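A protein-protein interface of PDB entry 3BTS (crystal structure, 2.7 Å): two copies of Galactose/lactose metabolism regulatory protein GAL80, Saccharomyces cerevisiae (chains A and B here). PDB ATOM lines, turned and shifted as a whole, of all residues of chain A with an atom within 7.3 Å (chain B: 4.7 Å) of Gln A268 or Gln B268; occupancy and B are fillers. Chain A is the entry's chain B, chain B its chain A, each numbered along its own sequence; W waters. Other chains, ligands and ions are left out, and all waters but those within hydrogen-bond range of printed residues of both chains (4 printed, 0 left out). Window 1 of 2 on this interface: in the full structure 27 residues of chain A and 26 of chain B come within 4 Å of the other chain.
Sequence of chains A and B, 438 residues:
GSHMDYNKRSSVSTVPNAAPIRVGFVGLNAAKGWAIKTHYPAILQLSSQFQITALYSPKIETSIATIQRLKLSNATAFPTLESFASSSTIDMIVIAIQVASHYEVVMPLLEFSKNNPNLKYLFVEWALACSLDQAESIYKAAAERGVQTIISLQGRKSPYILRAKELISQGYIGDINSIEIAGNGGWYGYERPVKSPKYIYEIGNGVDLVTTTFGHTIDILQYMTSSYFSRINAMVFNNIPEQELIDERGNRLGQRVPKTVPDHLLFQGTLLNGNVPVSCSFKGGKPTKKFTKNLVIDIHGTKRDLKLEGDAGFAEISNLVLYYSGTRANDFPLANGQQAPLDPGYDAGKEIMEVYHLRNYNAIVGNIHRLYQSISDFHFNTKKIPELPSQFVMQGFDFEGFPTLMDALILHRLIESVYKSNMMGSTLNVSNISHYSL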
ATOM      1  N   PHE A 214      15.867  -8.394  21.858  1.00  0.00           N
ATOM      2  CA  PHE A 214      14.422  -8.503  21.947  1.00  0.00           C
ATOM      3  C   PHE A 214      13.740  -7.130  22.019  1.00  0.00           C
ATOM      4  O   PHE A 214      12.666  -6.938  21.445  1.00  0.00           O
ATOM      5  CB  PHE A 214      14.051  -9.372  23.148  1.00  0.00           C
ATOM      6  CG  PHE A 214      12.630  -9.230  23.580  1.00  0.00           C
ATOM      7  CD1 PHE A 214      11.661 -10.084  23.090  1.00  0.00           C
ATOM      8  CD2 PHE A 214      12.257  -8.245  24.480  1.00  0.00           C
ATOM      9  CE1 PHE A 214      10.348  -9.965  23.489  1.00  0.00           C
ATOM     10  CE2 PHE A 214      10.937  -8.118  24.881  1.00  0.00           C
ATOM     11  CZ  PHE A 214       9.984  -8.980  24.380  1.00  0.00           C
ATOM     12  N   PHE A 229       0.827  -4.690  23.353  1.00  0.00           N
ATOM     13  CA  PHE A 229       0.368  -5.935  23.955  1.00  0.00           C
ATOM     14  C   PHE A 229      -0.663  -5.682  25.039  1.00  0.00           C
ATOM     15  O   PHE A 229      -0.690  -4.611  25.635  1.00  0.00           O
ATOM     16  CB  PHE A 229       1.555  -6.716  24.536  1.00  0.00           C
ATOM     17  CG  PHE A 229       2.456  -7.291  23.493  1.00  0.00           C
ATOM     18  CD1 PHE A 229       3.501  -6.546  22.983  1.00  0.00           C
ATOM     19  CD2 PHE A 229       2.233  -8.563  22.991  1.00  0.00           C
ATOM     20  CE1 PHE A 229       4.321  -7.064  22.002  1.00  0.00           C
ATOM     21  CE2 PHE A 229       3.048  -9.085  22.013  1.00  0.00           C
ATOM     22  CZ  PHE A 229       4.096  -8.335  21.519  1.00  0.00           C
ATOM     23  N   ARG A 231      -1.691  -8.817  27.156  1.00  0.00           N
ATOM     24  CA  ARG A 231      -1.184  -9.810  28.097  1.00  0.00           C
ATOM     25  C   ARG A 231       0.118 -10.402  27.573  1.00  0.00           C
ATOM     26  O   ARG A 231       0.285 -10.562  26.373  1.00  0.00           O
ATOM     27  CB  ARG A 231      -2.210 -10.924  28.333  1.00  0.00           C
ATOM     28  CG  ARG A 231      -3.611 -10.442  28.723  1.00  0.00           C
ATOM     29  CD  ARG A 231      -4.415 -11.567  29.376  1.00  0.00           C
ATOM     30  NE  ARG A 231      -4.281 -11.557  30.834  1.00  0.00           N
ATOM     31  CZ  ARG A 231      -4.286 -12.648  31.596  1.00  0.00           C
ATOM     32  NH1 ARG A 231      -4.401 -13.850  31.041  1.00  0.00           N
ATOM     33  NH2 ARG A 231      -4.161 -12.539  32.914  1.00  0.00           N
ATOM     34  N   ILE A 232       1.039 -10.720  28.473  1.00  0.00           N
ATOM     35  CA  ILE A 232       2.298 -11.349  28.087  1.00  0.00           C
ATOM     36  C   ILE A 232       2.766 -12.359  29.134  1.00  0.00           C
ATOM     37  O   ILE A 232       2.391 -12.273  30.299  1.00  0.00           O
ATOM     38  CB  ILE A 232       3.402 -10.304  27.840  1.00  0.00           C
ATOM     39  CG1 ILE A 232       3.760  -9.562  29.127  1.00  0.00           C
ATOM     40  CG2 ILE A 232       2.966  -9.307  26.794  1.00  0.00           C
ATOM     41  CD1 ILE A 232       5.019 -10.051  29.802  1.00  0.00           C
ATOM     42  N   ASN A 233       3.560 -13.330  28.708  1.00  0.00           N
ATOM     43  CA  ASN A 233       4.231 -14.233  29.640  1.00  0.00           C
ATOM     44  C   ASN A 233       5.624 -14.586  29.140  1.00  0.00           C
ATOM     45  O   ASN A 233       5.814 -14.916  27.967  1.00  0.00           O
ATOM     46  CB  ASN A 233       3.424 -15.510  29.895  1.00  0.00           C
ATOM     47  CG  ASN A 233       4.131 -16.464  30.857  1.00  0.00           C
ATOM     48  OD1 ASN A 233       5.088 -17.148  30.489  1.00  0.00           O
ATOM     49  ND2 ASN A 233       3.655 -16.512  32.096  1.00  0.00           N
ATOM     50  N   ALA A 234       6.593 -14.538  30.042  1.00  0.00           N
ATOM     51  CA  ALA A 234       7.983 -14.736  29.669  1.00  0.00           C
ATOM     52  C   ALA A 234       8.691 -15.714  30.585  1.00  0.00           C
ATOM     53  O   ALA A 234       8.461 -15.741  31.793  1.00  0.00           O
ATOM     54  CB  ALA A 234       8.717 -13.402  29.673  1.00  0.00           C
ATOM     55  N   MET A 235       9.556 -16.525  29.996  1.00  0.00           N
ATOM     56  CA  MET A 235      10.493 -17.308  30.777  1.00  0.00           C
ATOM     57  C   MET A 235      11.886 -16.925  30.302  1.00  0.00           C
ATOM     58  O   MET A 235      12.161 -16.947  29.106  1.00  0.00           O
ATOM     59  CB  MET A 235      10.236 -18.808  30.605  1.00  0.00           C
ATOM     60  CG  MET A 235       8.835 -19.228  31.004  1.00  0.00           C
ATOM     61  SD  MET A 235       8.479 -20.970  30.700  1.00  0.00           S
ATOM     62  CE  MET A 235       6.704 -20.992  30.939  1.00  0.00           C
ATOM     63  N   LEU A 265      15.375 -16.603  25.866  1.00  0.00           N
ATOM     64  CA  LEU A 265      14.142 -15.941  26.266  1.00  0.00           C
ATOM     65  C   LEU A 265      12.973 -16.581  25.525  1.00  0.00           C
ATOM     66  O   LEU A 265      12.995 -16.671  24.301  1.00  0.00           O
ATOM     67  CB  LEU A 265      14.209 -14.447  25.953  1.00  0.00           C
ATOM     68  CG  LEU A 265      12.860 -13.728  25.882  1.00  0.00           C
ATOM     69  CD1 LEU A 265      12.222 -13.647  27.246  1.00  0.00           C
ATOM     70  CD2 LEU A 265      13.016 -12.340  25.295  1.00  0.00           C
ATOM     71  N   LEU A 266      11.982 -17.057  26.273  1.00  0.00           N
ATOM     72  CA  LEU A 266      10.700 -17.467  25.704  1.00  0.00           C
ATOM     73  C   LEU A 266       9.680 -16.376  25.981  1.00  0.00           C
ATOM     74  O   LEU A 266       9.571 -15.885  27.109  1.00  0.00           O
ATOM     75  CB  LEU A 266      10.210 -18.770  26.325  1.00  0.00           C
ATOM     76  CG  LEU A 266      11.032 -20.027  26.066  1.00  0.00           C
ATOM     77  CD1 LEU A 266      10.405 -21.209  26.779  1.00  0.00           C
ATOM     78  CD2 LEU A 266      11.117 -20.295  24.590  1.00  0.00           C
ATOM     79  N   PHE A 267       8.930 -15.994  24.959  1.00  0.00           N
ATOM     80  CA  PHE A 267       7.957 -14.923  25.110  1.00  0.00           C
ATOM     81  C   PHE A 267       6.706 -15.219  24.310  1.00  0.00           C
ATOM     82  O   PHE A 267       6.775 -15.559  23.142  1.00  0.00           O
ATOM     83  CB  PHE A 267       8.570 -13.602  24.650  1.00  0.00           C
ATOM     84  CG  PHE A 267       7.582 -12.473  24.513  1.00  0.00           C
ATOM     85  CD1 PHE A 267       7.346 -11.602  25.567  1.00  0.00           C
ATOM     86  CD2 PHE A 267       6.912 -12.262  23.314  1.00  0.00           C
ATOM     87  CE1 PHE A 267       6.449 -10.550  25.438  1.00  0.00           C
ATOM     88  CE2 PHE A 267       6.014 -11.218  23.180  1.00  0.00           C
ATOM     89  CZ  PHE A 267       5.780 -10.363  24.240  1.00  0.00           C
ATOM     90  N   GLN A 268       5.558 -15.104  24.950  1.00  0.00           N
ATOM     91  CA  GLN A 268       4.296 -15.184  24.232  1.00  0.00           C
ATOM     92  C   GLN A 268       3.385 -14.079  24.746  1.00  0.00           C
ATOM     93  O   GLN A 268       3.502 -13.650  25.889  1.00  0.00           O
ATOM     94  CB  GLN A 268       3.658 -16.576  24.364  1.00  0.00           C
ATOM     95  CG  GLN A 268       3.378 -17.022  25.792  1.00  0.00           C
ATOM     96  CD  GLN A 268       3.088 -18.513  25.888  1.00  0.00           C
ATOM     97  OE1 GLN A 268       2.417 -18.968  26.811  1.00  0.00           O
ATOM     98  NE2 GLN A 268       3.599 -19.278  24.934  1.00  0.00           N
ATOM     99  N   GLY A 269       2.497 -13.596  23.891  1.00  0.00           N
ATOM    100  CA  GLY A 269       1.619 -12.516  24.288  1.00  0.00           C
ATOM    101  C   GLY A 269       0.516 -12.257  23.291  1.00  0.00           C
ATOM    102  O   GLY A 269       0.388 -12.959  22.302  1.00  0.00           O
ATOM    103  N   THR A 270      -0.289 -11.242  23.557  1.00  0.00           N
ATOM    104  CA  THR A 270      -1.375 -10.891  22.661  1.00  0.00           C
ATOM    105  C   THR A 270      -1.317  -9.417  22.345  1.00  0.00           C
ATOM    106  O   THR A 270      -1.065  -8.595  23.223  1.00  0.00           O
ATOM    107  CB  THR A 270      -2.761 -11.214  23.266  1.00  0.00           C
ATOM    108  OG1 THR A 270      -2.787 -10.822  24.639  1.00  0.00           O
ATOM    109  CG2 THR A 270      -3.041 -12.690  23.192  1.00  0.00           C
ATOM    110  N   PRO A 277      -2.267 -13.604  18.704  1.00  0.00           N
ATOM    111  CA  PRO A 277      -1.285 -14.468  19.372  1.00  0.00           C
ATOM    112  C   PRO A 277       0.126 -14.247  18.823  1.00  0.00           C
ATOM    113  O   PRO A 277       0.318 -14.194  17.611  1.00  0.00           O
ATOM    114  CB  PRO A 277      -1.765 -15.881  19.024  1.00  0.00           C
ATOM    115  CG  PRO A 277      -3.174 -15.720  18.564  1.00  0.00           C
ATOM    116  CD  PRO A 277      -3.228 -14.380  17.908  1.00  0.00           C
ATOM    117  N   VAL A 278       1.098 -14.129  19.714  1.00  0.00           N
ATOM    118  CA  VAL A 278       2.481 -13.887  19.328  1.00  0.00           C
ATOM    119  C   VAL A 278       3.406 -14.842  20.077  1.00  0.00           C
ATOM    120  O   VAL A 278       3.503 -14.792  21.299  1.00  0.00           O
ATOM    121  CB  VAL A 278       2.891 -12.438  19.672  1.00  0.00           C
ATOM    122  CG1 VAL A 278       4.313 -12.152  19.234  1.00  0.00           C
ATOM    123  CG2 VAL A 278       1.934 -11.455  19.050  1.00  0.00           C
ATOM    124  N   SER A 279       4.078 -15.706  19.332  1.00  0.00           N
ATOM    125  CA  SER A 279       5.008 -16.667  19.898  1.00  0.00           C
ATOM    126  C   SER A 279       6.417 -16.244  19.562  1.00  0.00           C
ATOM    127  O   SER A 279       6.726 -15.969  18.404  1.00  0.00           O
ATOM    128  CB  SER A 279       4.752 -18.060  19.311  1.00  0.00           C
ATOM    129  OG  SER A 279       5.520 -19.038  19.992  1.00  0.00           O
ATOM    130  N   CYS A 280       7.282 -16.184  20.567  1.00  0.00           N
ATOM    131  CA  CYS A 280       8.644 -15.712  20.346  1.00  0.00           C
ATOM    132  C   CYS A 280       9.676 -16.539  21.085  1.00  0.00           C
ATOM    133  O   CYS A 280       9.478 -16.934  22.233  1.00  0.00           O
ATOM    134  CB  CYS A 280       8.780 -14.242  20.746  1.00  0.00           C
ATOM    135  SG  CYS A 280       7.589 -13.153  19.936  1.00  0.00           S
ATOM    136  N   SER A 281      10.785 -16.791  20.409  1.00  0.00           N
ATOM    137  CA  SER A 281      11.909 -17.495  21.005  1.00  0.00           C
ATOM    138  C   SER A 281      13.216 -16.789  20.644  1.00  0.00           C
ATOM    139  O   SER A 281      13.469 -16.512  19.475  1.00  0.00           O
ATOM    140  CB  SER A 281      11.945 -18.946  20.538  1.00  0.00           C
ATOM    141  OG  SER A 281      12.904 -19.670  21.282  1.00  0.00           O
ATOM    142  N   SER A 421       7.320 -10.878  34.814  1.00  0.00           N
ATOM    143  CA  SER A 421       6.558 -12.074  34.470  1.00  0.00           C
ATOM    144  C   SER A 421       7.336 -13.337  34.785  1.00  0.00           C
ATOM    145  O   SER A 421       6.791 -14.282  35.348  1.00  0.00           O
ATOM    146  CB  SER A 421       6.180 -12.068  32.993  1.00  0.00           C
ATOM    147  OG  SER A 421       5.569 -13.291  32.630  1.00  0.00           O
ATOM    148  N   THR A 427       1.248 -14.552  34.042  1.00  0.00           N
ATOM    149  CA  THR A 427       0.890 -13.789  32.857  1.00  0.00           C
ATOM    150  C   THR A 427       0.363 -12.412  33.244  1.00  0.00           C
ATOM    151  O   THR A 427      -0.624 -12.298  33.974  1.00  0.00           O
ATOM    152  CB  THR A 427      -0.162 -14.539  32.040  1.00  0.00           C
ATOM    153  OG1 THR A 427       0.408 -15.765  31.570  1.00  0.00           O
ATOM    154  CG2 THR A 427      -0.622 -13.704  30.864  1.00  0.00           C
ATOM    155  N   ARG B 231       7.942 -26.956  34.042  1.00  0.00           N
ATOM    156  CA  ARG B 231       7.094 -25.766  34.086  1.00  0.00           C
ATOM    157  C   ARG B 231       6.506 -25.506  32.712  1.00  0.00           C
ATOM    158  O   ARG B 231       7.154 -25.760  31.709  1.00  0.00           O
ATOM    159  CB  ARG B 231       7.873 -24.527  34.558  1.00  0.00           C
ATOM    160  CG  ARG B 231       8.658 -24.705  35.855  1.00  0.00           C
ATOM    161  CD  ARG B 231       9.011 -23.357  36.456  1.00  0.00           C
ATOM    162  NE  ARG B 231       7.992 -22.895  37.396  1.00  0.00           N
ATOM    163  CZ  ARG B 231       7.673 -21.619  37.592  1.00  0.00           C
ATOM    164  NH1 ARG B 231       8.281 -20.666  36.895  1.00  0.00           N
ATOM    165  NH2 ARG B 231       6.734 -21.297  38.475  1.00  0.00           N
ATOM    166  N   ILE B 232       5.281 -24.993  32.667  1.00  0.00           N
ATOM    167  CA  ILE B 232       4.647 -24.662  31.398  1.00  0.00           C
ATOM    168  C   ILE B 232       3.792 -23.401  31.521  1.00  0.00           C
ATOM    169  O   ILE B 232       3.363 -23.038  32.619  1.00  0.00           O
ATOM    170  CB  ILE B 232       3.782 -25.843  30.860  1.00  0.00           C
ATOM    171  CG1 ILE B 232       2.620 -26.151  31.804  1.00  0.00           C
ATOM    172  CG2 ILE B 232       4.616 -27.094  30.651  1.00  0.00           C
ATOM    173  CD1 ILE B 232       1.307 -25.564  31.349  1.00  0.00           C
ATOM    174  N   ASN B 233       3.561 -22.730  30.395  1.00  0.00           N
ATOM    175  CA  ASN B 233       2.579 -21.652  30.341  1.00  0.00           C
ATOM    176  C   ASN B 233       1.868 -21.634  29.008  1.00  0.00           C
ATOM    177  O   ASN B 233       2.489 -21.771  27.961  1.00  0.00           O
ATOM    178  CB  ASN B 233       3.202 -20.288  30.614  1.00  0.00           C
ATOM    179  CG  ASN B 233       2.178 -19.160  30.559  1.00  0.00           C
ATOM    180  OD1 ASN B 233       1.747 -18.753  29.483  1.00  0.00           O
ATOM    181  ND2 ASN B 233       1.797 -18.643  31.723  1.00  0.00           N
ATOM    182  N   ALA B 234       0.555 -21.453  29.057  1.00  0.00           N
ATOM    183  CA  ALA B 234      -0.269 -21.563  27.868  1.00  0.00           C
ATOM    184  C   ALA B 234      -1.252 -20.421  27.750  1.00  0.00           C
ATOM    185  O   ALA B 234      -1.828 -19.984  28.735  1.00  0.00           O
ATOM    186  CB  ALA B 234      -1.017 -22.900  27.870  1.00  0.00           C
ATOM    187  N   MET B 235      -1.442 -19.945  26.529  1.00  0.00           N
ATOM    188  CA  MET B 235      -2.553 -19.058  26.234  1.00  0.00           C
ATOM    189  C   MET B 235      -3.380 -19.725  25.150  1.00  0.00           C
ATOM    190  O   MET B 235      -2.839 -20.161  24.129  1.00  0.00           O
ATOM    191  CB  MET B 235      -2.055 -17.681  25.796  1.00  0.00           C
ATOM    192  CG  MET B 235      -1.195 -16.988  26.853  1.00  0.00           C
ATOM    193  SD  MET B 235      -0.482 -15.435  26.300  1.00  0.00           S
ATOM    194  CE  MET B 235       0.758 -15.161  27.563  1.00  0.00           C
ATOM    195  N   LEU B 266      -0.942 -20.919  22.184  1.00  0.00           N
ATOM    196  CA  LEU B 266       0.453 -20.590  22.473  1.00  0.00           C
ATOM    197  C   LEU B 266       0.915 -21.431  23.648  1.00  0.00           C
ATOM    198  O   LEU B 266       0.226 -21.522  24.663  1.00  0.00           O
ATOM    199  CB  LEU B 266       0.596 -19.113  22.826  1.00  0.00           C
ATOM    200  CG  LEU B 266       0.327 -18.100  21.715  1.00  0.00           C
ATOM    201  CD1 LEU B 266       0.521 -16.709  22.248  1.00  0.00           C
ATOM    202  CD2 LEU B 266       1.236 -18.334  20.522  1.00  0.00           C
ATOM    203  N   PHE B 267       2.078 -22.052  23.516  1.00  0.00           N
ATOM    204  CA  PHE B 267       2.592 -22.897  24.584  1.00  0.00           C
ATOM    205  C   PHE B 267       4.094 -22.748  24.712  1.00  0.00           C
ATOM    206  O   PHE B 267       4.817 -22.824  23.726  1.00  0.00           O
ATOM    207  CB  PHE B 267       2.225 -24.356  24.312  1.00  0.00           C
ATOM    208  CG  PHE B 267       2.934 -25.347  25.194  1.00  0.00           C
ATOM    209  CD1 PHE B 267       2.352 -25.789  26.364  1.00  0.00           C
ATOM    210  CD2 PHE B 267       4.164 -25.861  24.837  1.00  0.00           C
ATOM    211  CE1 PHE B 267       2.986 -26.710  27.167  1.00  0.00           C
ATOM    212  CE2 PHE B 267       4.802 -26.780  25.636  1.00  0.00           C
ATOM    213  CZ  PHE B 267       4.209 -27.208  26.803  1.00  0.00           C
ATOM    214  N   GLN B 268       4.562 -22.516  25.927  1.00  0.00           N
ATOM    215  CA  GLN B 268       5.993 -22.563  26.193  1.00  0.00           C
ATOM    216  C   GLN B 268       6.239 -23.314  27.485  1.00  0.00           C
ATOM    217  O   GLN B 268       5.387 -23.323  28.376  1.00  0.00           O
ATOM    218  CB  GLN B 268       6.586 -21.158  26.249  1.00  0.00           C
ATOM    219  CG  GLN B 268       5.943 -20.236  27.253  1.00  0.00           C
ATOM    220  CD  GLN B 268       6.316 -18.779  27.033  1.00  0.00           C
ATOM    221  OE1 GLN B 268       6.288 -17.980  27.967  1.00  0.00           O
ATOM    222  NE2 GLN B 268       6.666 -18.429  25.794  1.00  0.00           N
ATOM    223  N   GLY B 269       7.391 -23.963  27.588  1.00  0.00           N
ATOM    224  CA  GLY B 269       7.688 -24.744  28.777  1.00  0.00           C
ATOM    225  C   GLY B 269       9.137 -25.169  28.861  1.00  0.00           C
ATOM    226  O   GLY B 269       9.967 -24.754  28.059  1.00  0.00           O
ATOM    227  N   VAL B 278      11.145 -24.674  25.340  1.00  0.00           N
ATOM    228  CA  VAL B 278      10.286 -25.184  24.285  1.00  0.00           C
ATOM    229  C   VAL B 278       9.243 -24.137  23.907  1.00  0.00           C
ATOM    230  O   VAL B 278       8.399 -23.768  24.721  1.00  0.00           O
ATOM    231  CB  VAL B 278       9.573 -26.481  24.717  1.00  0.00           C
ATOM    232  CG1 VAL B 278       8.733 -27.039  23.565  1.00  0.00           C
ATOM    233  CG2 VAL B 278      10.580 -27.511  25.228  1.00  0.00           C
ATOM    234  N   SER B 279       9.316 -23.656  22.672  1.00  0.00           N
ATOM    235  CA  SER B 279       8.368 -22.665  22.172  1.00  0.00           C
ATOM    236  C   SER B 279       7.439 -23.315  21.155  1.00  0.00           C
ATOM    237  O   SER B 279       7.888 -23.966  20.215  1.00  0.00           O
ATOM    238  CB  SER B 279       9.107 -21.499  21.524  1.00  0.00           C
ATOM    239  OG  SER B 279       8.232 -20.427  21.244  1.00  0.00           O
HETATM  240  O   HOH W   1       4.457 -19.677  22.489  1.00  0.00           O
HETATM  241  O   HOH W   2       7.159 -18.865  23.406  1.00  0.00           O
HETATM  242  O   HOH W   3       7.368 -20.000  18.617  1.00  0.00           O
HETATM  243  O   HOH W   4      -1.165 -17.672  30.932  1.00  0.00           O
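Ile A232 touches Met B235, and with the chains exchanged Met A235 touches Ile B232. Asn A233 touches Met B235, and with the chains exchanged Met A235 touches Asn B233. Leu A266 touches Gln B268, and with the chains exchanged Gln A268 touches Leu B266. Leu A266 touches Ser B279, and with the chains exchanged Ser A279 touches Leu B266. Of the 26 pairs that touch across the chains among the printed residues, 21 have their exchanged pair printed and touching as well.
Among the printed residues, merely in contact across the chains: Asn A233 with Met B235, Gln A268 with Met B235, Met A235 with Asn B233, Leu A266 with Gln B268, Val A278 with Leu B266, Gln A268 with Leu B266, Met A235 with Gln B268, Ser A279 with Leu B266, Gly A269 with Leu B266, Ile A232 with Met B235, Leu A266 with Gly B269, Met A235 with Ile B232, Leu A266 with Val B278, Gln A268 with Ala B234, Cys A280 with Ser B279, Leu A266 with Ser B279, Thr A427 with Met B235 and Ser A281 with Ser B279.
The backbone NH (N) of Phe A267 lies close to the side-chain amide nitrogen (NE2) of Gln B268 (3.4 Å). The side-chain hydroxyl (OG) of Ser B279 is in hydrogen-bond range of the side-chain hydroxyl (OG) of Ser A279 (3.3 Å). The backbone NH (N) of Phe B267 lies close to the side-chain amide nitrogen (NE2) of Gln A268, 3.5 Å away. The side-chain hydroxyl of Thr A427 sits at hydrogen-bond distance from the side-chain amide nitrogen of Asn B233 (3.2 Å). The side-chain amide oxygen of Asn B233 sits close to the side-chain amide oxygen of Gln A268 (2.8 Å). The side-chain amide nitrogen (NE2) of Gln B268 lies close to the side-chain amide nitrogen (NE2) of Gln A268 (3.3 Å). ND2 of Asn A233 sits close to ND2 of Asn B233 (2.9 Å). The side-chain amide oxygen of Gln B268 sits close to the side-chain amide oxygen of Asn A233 (2.9 Å).
Gln A268 touches just these residues of chain B: Asn B233, Ala B234, Met B235, Leu B266, Phe B267 and Gln B268. Gln B268 touches just these residues of chain A: Asn A233 (2.9 Å), Met A235 (3.7 Å), Leu A266 (3.6 Å), Phe A267 (3.4 Å) and Gln A268 (3.3 Å). Of the printed residues of chain A, Met B235 touches Ile A232 (3.8 Å), Asn A233 (3.5 Å), Gln A268 (3.6 Å) and Thr A427 (3.9 Å). Of the printed residues of chain A, Phe B267 touches Gln A268. Of the printed residues of chain B, Thr A427 touches Asn B233 and Met B235. Of the printed residues of chain B, Asn A233 touches Asn B233, Met B235 and Gln B268. Of the printed residues of chain A, Asn B233 touches Asn A233 (2.9 Å), Met A235 (3.6 Å), Gln A268 (2.8 Å) and Thr A427 (3.2 Å). Arg A231 touches none of the printed residues of chain B. The nearest printed residue of chain B that does not touch Val A278 is Met B235 (6.4 Å).
The backbone NH (N) of Asn A233 sits at hydrogen-bond distance from the backbone carbonyl oxygen (O) of Gln A268 (2.8 Å). N of Leu B266 sits at hydrogen-bond distance from O of Met B235 (2.8 Å). The backbone NH of Asn B233 is in hydrogen-bond range of the backbone carbonyl oxygen of Gln B268 (2.8 Å). The side-chain amide nitrogen (ND2) of Asn A233 sits at hydrogen-bond distance from the side-chain hydroxyl (OG1) of Thr A427 (3.4 Å). N of Val B278 is in hydrogen-bond range of O of Gly B269 (3.0 Å). The backbone carbonyl oxygen (O) of Gly A269 lies within hydrogen-bond range of the backbone NH (N) of Val A278, at 2.9 Å.
Water W2 lies within hydrogen-bond range of NE2 of Gln B268 (2.5 Å), OG of Ser B279 (2.9 Å), O of Cys A280 (3.2 Å) and O of Phe A267 (3.3 Å). Water W3 lies within hydrogen-bond range of OG of Ser A279 and OG of Ser B279. Water W4 lies within hydrogen-bond range of OG1 of Thr A427, ND2 of Asn B233 and O of Ala B234. Water W1 lies within hydrogen-bond range of the side-chain amide nitrogen (NE2) of Gln A268, the side-chain hydroxyl (OG) of Ser A279 and the backbone carbonyl oxygen (O) of Phe B267.
Of the 11 printed residues of chain B, 10 touch a printed residue of chain A. Among the printed residues, 26 pairs touch across the chains. Among the printed residues, no Asp or Glu carboxylate lies within 4 Å of a Lys or Arg side-chain nitrogen of the other chain.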
